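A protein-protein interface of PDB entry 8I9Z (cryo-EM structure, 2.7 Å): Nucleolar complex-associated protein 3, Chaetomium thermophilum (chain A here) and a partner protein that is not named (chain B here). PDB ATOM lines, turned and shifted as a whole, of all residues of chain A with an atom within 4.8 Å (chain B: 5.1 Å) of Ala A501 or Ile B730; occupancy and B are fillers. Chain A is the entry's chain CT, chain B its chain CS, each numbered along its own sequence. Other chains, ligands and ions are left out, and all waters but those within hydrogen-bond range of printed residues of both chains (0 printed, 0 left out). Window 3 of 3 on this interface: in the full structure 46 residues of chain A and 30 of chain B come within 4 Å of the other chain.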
ATOM      1  N   HIS A 432      27.741   8.178  24.782  1.00  0.00           N
ATOM      2  CA  HIS A 432      26.404   8.705  24.567  1.00  0.00           C
ATOM      3  C   HIS A 432      25.309   7.728  24.966  1.00  0.00           C
ATOM      4  O   HIS A 432      24.148   8.135  25.076  1.00  0.00           O
ATOM      5  CB  HIS A 432      26.245   9.123  23.107  1.00  0.00           C
ATOM      6  CG  HIS A 432      26.175   7.976  22.152  1.00  0.00           C
ATOM      7  ND1 HIS A 432      27.269   7.203  21.838  1.00  0.00           N
ATOM      8  CD2 HIS A 432      25.145   7.481  21.428  1.00  0.00           C
ATOM      9  CE1 HIS A 432      26.917   6.275  20.968  1.00  0.00           C
ATOM     10  NE2 HIS A 432      25.632   6.421  20.702  1.00  0.00           N
ATOM     11  N   ILE A 434      25.455   5.985  27.916  1.00  0.00           N
ATOM     12  CA  ILE A 434      25.398   6.048  29.373  1.00  0.00           C
ATOM     13  C   ILE A 434      24.676   7.308  29.826  1.00  0.00           C
ATOM     14  O   ILE A 434      24.371   8.183  29.009  1.00  0.00           O
ATOM     15  CB  ILE A 434      26.815   5.932  29.963  1.00  0.00           C
ATOM     16  CG1 ILE A 434      27.494   7.292  30.094  1.00  0.00           C
ATOM     17  CG2 ILE A 434      27.651   5.000  29.119  1.00  0.00           C
ATOM     18  CD1 ILE A 434      28.724   7.243  30.950  1.00  0.00           C
ATOM     19  N   GLN A 436      23.126  10.800  31.404  1.00  0.00           N
ATOM     20  CA  GLN A 436      23.427  12.187  31.071  1.00  0.00           C
ATOM     21  C   GLN A 436      24.330  12.854  32.095  1.00  0.00           C
ATOM     22  O   GLN A 436      25.185  13.668  31.734  1.00  0.00           O
ATOM     23  CB  GLN A 436      22.125  12.979  30.943  1.00  0.00           C
ATOM     24  CG  GLN A 436      22.296  14.394  30.475  1.00  0.00           C
ATOM     25  CD  GLN A 436      20.996  15.016  30.050  1.00  0.00           C
ATOM     26  OE1 GLN A 436      19.965  14.366  30.067  1.00  0.00           O
ATOM     27  NE2 GLN A 436      21.039  16.283  29.664  1.00  0.00           N
ATOM     28  N   PHE A 439      28.167  12.291  31.665  1.00  0.00           N
ATOM     29  CA  PHE A 439      28.885  12.843  30.522  1.00  0.00           C
ATOM     30  C   PHE A 439      29.835  13.951  30.951  1.00  0.00           C
ATOM     31  O   PHE A 439      30.954  14.056  30.436  1.00  0.00           O
ATOM     32  CB  PHE A 439      27.902  13.353  29.476  1.00  0.00           C
ATOM     33  CG  PHE A 439      28.403  13.223  28.074  1.00  0.00           C
ATOM     34  CD1 PHE A 439      29.134  14.238  27.491  1.00  0.00           C
ATOM     35  CD2 PHE A 439      28.156  12.075  27.346  1.00  0.00           C
ATOM     36  CE1 PHE A 439      29.599  14.113  26.203  1.00  0.00           C
ATOM     37  CE2 PHE A 439      28.619  11.947  26.060  1.00  0.00           C
ATOM     38  CZ  PHE A 439      29.340  12.965  25.488  1.00  0.00           C
ATOM     39  N   ASP A 497      24.427  14.178  19.490  1.00  0.00           N
ATOM     40  CA  ASP A 497      23.580  14.393  20.658  1.00  0.00           C
ATOM     41  C   ASP A 497      24.300  15.204  21.726  1.00  0.00           C
ATOM     42  O   ASP A 497      23.677  16.008  22.429  1.00  0.00           O
ATOM     43  CB  ASP A 497      23.117  13.053  21.222  1.00  0.00           C
ATOM     44  CG  ASP A 497      24.171  11.976  21.103  1.00  0.00           C
ATOM     45  OD1 ASP A 497      25.301  12.294  20.676  1.00  0.00           O
ATOM     46  OD2 ASP A 497      23.872  10.810  21.436  1.00  0.00           O
ATOM     47  N   ALA A 498      25.612  15.010  21.864  1.00  0.00           N
ATOM     48  CA  ALA A 498      26.376  15.784  22.833  1.00  0.00           C
ATOM     49  C   ALA A 498      26.529  17.229  22.394  1.00  0.00           C
ATOM     50  O   ALA A 498      26.634  18.126  23.236  1.00  0.00           O
ATOM     51  CB  ALA A 498      27.748  15.148  23.045  1.00  0.00           C
ATOM     52  N   HIS A 499      26.558  17.471  21.083  1.00  0.00           N
ATOM     53  CA  HIS A 499      26.708  18.830  20.578  1.00  0.00           C
ATOM     54  C   HIS A 499      25.476  19.673  20.874  1.00  0.00           C
ATOM     55  O   HIS A 499      25.590  20.864  21.184  1.00  0.00           O
ATOM     56  CB  HIS A 499      26.986  18.797  19.080  1.00  0.00           C
ATOM     57  CG  HIS A 499      26.911  20.139  18.430  1.00  0.00           C
ATOM     58  ND1 HIS A 499      27.902  21.084  18.561  1.00  0.00           N
ATOM     59  CD2 HIS A 499      25.957  20.698  17.650  1.00  0.00           C
ATOM     60  CE1 HIS A 499      27.562  22.169  17.890  1.00  0.00           C
ATOM     61  NE2 HIS A 499      26.389  21.960  17.325  1.00  0.00           N
ATOM     62  N   ASN A 500      24.289  19.075  20.788  1.00  0.00           N
ATOM     63  CA  ASN A 500      23.069  19.804  21.100  1.00  0.00           C
ATOM     64  C   ASN A 500      22.889  20.025  22.595  1.00  0.00           C
ATOM     65  O   ASN A 500      22.001  20.785  22.992  1.00  0.00           O
ATOM     66  CB  ASN A 500      21.861  19.066  20.529  1.00  0.00           C
ATOM     67  CG  ASN A 500      21.824  19.103  19.022  1.00  0.00           C
ATOM     68  OD1 ASN A 500      22.736  18.623  18.357  1.00  0.00           O
ATOM     69  ND2 ASN A 500      20.765  19.678  18.472  1.00  0.00           N
ATOM     70  N   ALA A 501      23.703  19.384  23.428  1.00  0.00           N
ATOM     71  CA  ALA A 501      23.623  19.532  24.872  1.00  0.00           C
ATOM     72  C   ALA A 501      24.787  20.316  25.460  1.00  0.00           C
ATOM     73  O   ALA A 501      25.112  20.122  26.634  1.00  0.00           O
ATOM     74  CB  ALA A 501      23.542  18.156  25.535  1.00  0.00           C
ATOM     75  N   ARG A 502      25.435  21.175  24.673  1.00  0.00           N
ATOM     76  CA  ARG A 502      26.478  22.044  25.208  1.00  0.00           C
ATOM     77  C   ARG A 502      25.901  23.066  26.175  1.00  0.00           C
ATOM     78  O   ARG A 502      26.527  23.414  27.181  1.00  0.00           O
ATOM     79  CB  ARG A 502      27.191  22.762  24.067  1.00  0.00           C
ATOM     80  CG  ARG A 502      27.986  21.887  23.150  1.00  0.00           C
ATOM     81  CD  ARG A 502      28.350  22.696  21.933  1.00  0.00           C
ATOM     82  NE  ARG A 502      27.154  23.298  21.357  1.00  0.00           N
ATOM     83  CZ  ARG A 502      27.149  24.381  20.597  1.00  0.00           C
ATOM     84  NH1 ARG A 502      28.264  25.028  20.308  1.00  0.00           N
ATOM     85  NH2 ARG A 502      25.995  24.829  20.115  1.00  0.00           N
ATOM     86  N   SER A 503      24.720  23.596  25.859  1.00  0.00           N
ATOM     87  CA  SER A 503      24.114  24.602  26.722  1.00  0.00           C
ATOM     88  C   SER A 503      23.595  23.977  28.010  1.00  0.00           C
ATOM     89  O   SER A 503      23.818  24.510  29.103  1.00  0.00           O
ATOM     90  CB  SER A 503      22.987  25.316  25.977  1.00  0.00           C
ATOM     91  OG  SER A 503      22.342  24.442  25.068  1.00  0.00           O
ATOM     92  N   ASP A 504      22.906  22.841  27.899  1.00  0.00           N
ATOM     93  CA  ASP A 504      22.318  22.207  29.073  1.00  0.00           C
ATOM     94  C   ASP A 504      23.391  21.564  29.938  1.00  0.00           C
ATOM     95  O   ASP A 504      23.590  21.951  31.095  1.00  0.00           O
ATOM     96  CB  ASP A 504      21.279  21.175  28.637  1.00  0.00           C
ATOM     97  CG  ASP A 504      20.351  21.703  27.566  1.00  0.00           C
ATOM     98  OD1 ASP A 504      20.439  22.905  27.246  1.00  0.00           O
ATOM     99  OD2 ASP A 504      19.534  20.916  27.044  1.00  0.00           O
ATOM    100  N   LEU A 505      24.095  20.581  29.394  1.00  0.00           N
ATOM    101  CA  LEU A 505      25.249  20.001  30.065  1.00  0.00           C
ATOM    102  C   LEU A 505      26.423  20.943  29.861  1.00  0.00           C
ATOM    103  O   LEU A 505      26.897  21.107  28.733  1.00  0.00           O
ATOM    104  CB  LEU A 505      25.561  18.622  29.496  1.00  0.00           C
ATOM    105  CG  LEU A 505      24.612  17.467  29.774  1.00  0.00           C
ATOM    106  CD1 LEU A 505      25.367  16.177  29.575  1.00  0.00           C
ATOM    107  CD2 LEU A 505      24.054  17.558  31.180  1.00  0.00           C
ATOM    108  N   LEU A 507      29.409  21.693  29.138  1.00  0.00           N
ATOM    109  CA  LEU A 507      30.590  21.012  28.624  1.00  0.00           C
ATOM    110  C   LEU A 507      31.437  22.048  27.897  1.00  0.00           C
ATOM    111  O   LEU A 507      31.208  22.331  26.718  1.00  0.00           O
ATOM    112  CB  LEU A 507      30.192  19.866  27.700  1.00  0.00           C
ATOM    113  CG  LEU A 507      29.265  18.809  28.302  1.00  0.00           C
ATOM    114  CD1 LEU A 507      28.481  18.113  27.211  1.00  0.00           C
ATOM    115  CD2 LEU A 507      30.033  17.799  29.129  1.00  0.00           C
ATOM    116  N   ARG B 728      18.981   7.288  31.717  1.00  0.00           N
ATOM    117  CA  ARG B 728      18.807   8.708  31.409  1.00  0.00           C
ATOM    118  C   ARG B 728      19.929   9.221  30.514  1.00  0.00           C
ATOM    119  O   ARG B 728      20.760  10.025  30.949  1.00  0.00           O
ATOM    120  CB  ARG B 728      18.766   9.511  32.709  1.00  0.00           C
ATOM    121  CG  ARG B 728      17.757  10.612  32.759  1.00  0.00           C
ATOM    122  CD  ARG B 728      17.855  11.348  34.076  1.00  0.00           C
ATOM    123  NE  ARG B 728      18.883  12.378  34.046  1.00  0.00           N
ATOM    124  CZ  ARG B 728      18.636  13.662  33.837  1.00  0.00           C
ATOM    125  NH1 ARG B 728      17.406  14.103  33.635  1.00  0.00           N
ATOM    126  NH2 ARG B 728      19.647  14.525  33.835  1.00  0.00           N
ATOM    127  N   PRO B 729      19.980   8.802  29.252  1.00  0.00           N
ATOM    128  CA  PRO B 729      21.006   9.334  28.356  1.00  0.00           C
ATOM    129  C   PRO B 729      20.511  10.568  27.610  1.00  0.00           C
ATOM    130  O   PRO B 729      19.345  10.955  27.703  1.00  0.00           O
ATOM    131  CB  PRO B 729      21.272   8.165  27.403  1.00  0.00           C
ATOM    132  CG  PRO B 729      20.006   7.460  27.328  1.00  0.00           C
ATOM    133  CD  PRO B 729      19.209   7.741  28.580  1.00  0.00           C
ATOM    134  N   ILE B 730      21.437  11.189  26.871  1.00  0.00           N
ATOM    135  CA  ILE B 730      21.161  12.474  26.227  1.00  0.00           C
ATOM    136  C   ILE B 730      20.096  12.320  25.153  1.00  0.00           C
ATOM    137  O   ILE B 730      19.279  13.222  24.933  1.00  0.00           O
ATOM    138  CB  ILE B 730      22.458  13.082  25.656  1.00  0.00           C
ATOM    139  CG1 ILE B 730      23.537  13.147  26.733  1.00  0.00           C
ATOM    140  CG2 ILE B 730      22.214  14.477  25.117  1.00  0.00           C
ATOM    141  CD1 ILE B 730      24.834  13.741  26.253  1.00  0.00           C
ATOM    142  N   LYS B 731      20.082  11.175  24.473  1.00  0.00           N
ATOM    143  CA  LYS B 731      19.110  10.957  23.409  1.00  0.00           C
ATOM    144  C   LYS B 731      17.694  10.882  23.964  1.00  0.00           C
ATOM    145  O   LYS B 731      16.791  11.559  23.467  1.00  0.00           O
ATOM    146  CB  LYS B 731      19.463   9.691  22.634  1.00  0.00           C
ATOM    147  CG  LYS B 731      18.657   9.498  21.369  1.00  0.00           C
ATOM    148  CD  LYS B 731      19.532   8.991  20.235  1.00  0.00           C
ATOM    149  CE  LYS B 731      20.303   7.743  20.637  1.00  0.00           C
ATOM    150  NZ  LYS B 731      21.032   7.134  19.490  1.00  0.00           N
ATOM    151  N   LYS B 732      17.484  10.088  25.018  1.00  0.00           N
ATOM    152  CA  LYS B 732      16.127   9.873  25.516  1.00  0.00           C
ATOM    153  C   LYS B 732      15.592  11.094  26.253  1.00  0.00           C
ATOM    154  O   LYS B 732      14.386  11.360  26.223  1.00  0.00           O
ATOM    155  CB  LYS B 732      16.081   8.642  26.414  1.00  0.00           C
ATOM    156  CG  LYS B 732      16.703   7.406  25.783  1.00  0.00           C
ATOM    157  CD  LYS B 732      16.384   6.073  26.490  1.00  0.00           C
ATOM    158  CE  LYS B 732      15.017   5.960  27.191  1.00  0.00           C
ATOM    159  NZ  LYS B 732      13.814   6.429  26.421  1.00  0.00           N
ATOM    160  N   VAL B 733      16.462  11.841  26.928  1.00  0.00           N
ATOM    161  CA  VAL B 733      16.032  13.075  27.575  1.00  0.00           C
ATOM    162  C   VAL B 733      15.640  14.116  26.531  1.00  0.00           C
ATOM    163  O   VAL B 733      14.713  14.906  26.738  1.00  0.00           O
ATOM    164  CB  VAL B 733      17.137  13.569  28.526  1.00  0.00           C
ATOM    165  CG1 VAL B 733      16.845  14.960  29.068  1.00  0.00           C
ATOM    166  CG2 VAL B 733      17.285  12.595  29.669  1.00  0.00           C
ATOM    167  N   ALA B 734      16.320  14.114  25.381  1.00  0.00           N
ATOM    168  CA  ALA B 734      15.999  15.067  24.323  1.00  0.00           C
ATOM    169  C   ALA B 734      14.632  14.792  23.699  1.00  0.00           C
ATOM    170  O   ALA B 734      13.848  15.723  23.484  1.00  0.00           O
ATOM    171  CB  ALA B 734      17.088  15.046  23.254  1.00  0.00           C
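Among the printed residues, 8 pairs touch across the chains.
Among the printed residues, no Asp or Glu carboxylate lies within 4 Å of a Lys or Arg side-chain nitrogen of the other chain.
Of chain B, only Ile B730 comes within 4 Å of Ala A501.
Ile B730 touches just these residues of chain A: Phe A439 (3.9 Å), Asp A497 (3.4 Å) and Ala A501 (3.9 Å).
Of the printed residues of chain B, Gln A436 touches Arg B728, Pro B729 and Val B733.
Of the printed residues of chain A, Val B733 touches Gln A436.
Of the printed residues of chain B, His A432 touches Pro B729 (3.7 Å).
The nearest printed residue of chain B that does not touch Ala A501 is Ala B734 (7.5 Å).
Among the printed residues, merely in contact across the chains: His A432 with Pro B729, Ile A434 with Pro B729, Gln A436 with Pro B729, Gln A436 with Val B733, Phe A439 with Ile B730, Asp A497 with Ile B730 and Ala A501 with Ile B730.
N of Gln A436 is in hydrogen-bond range of O of Arg B728 (2.5 Å).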
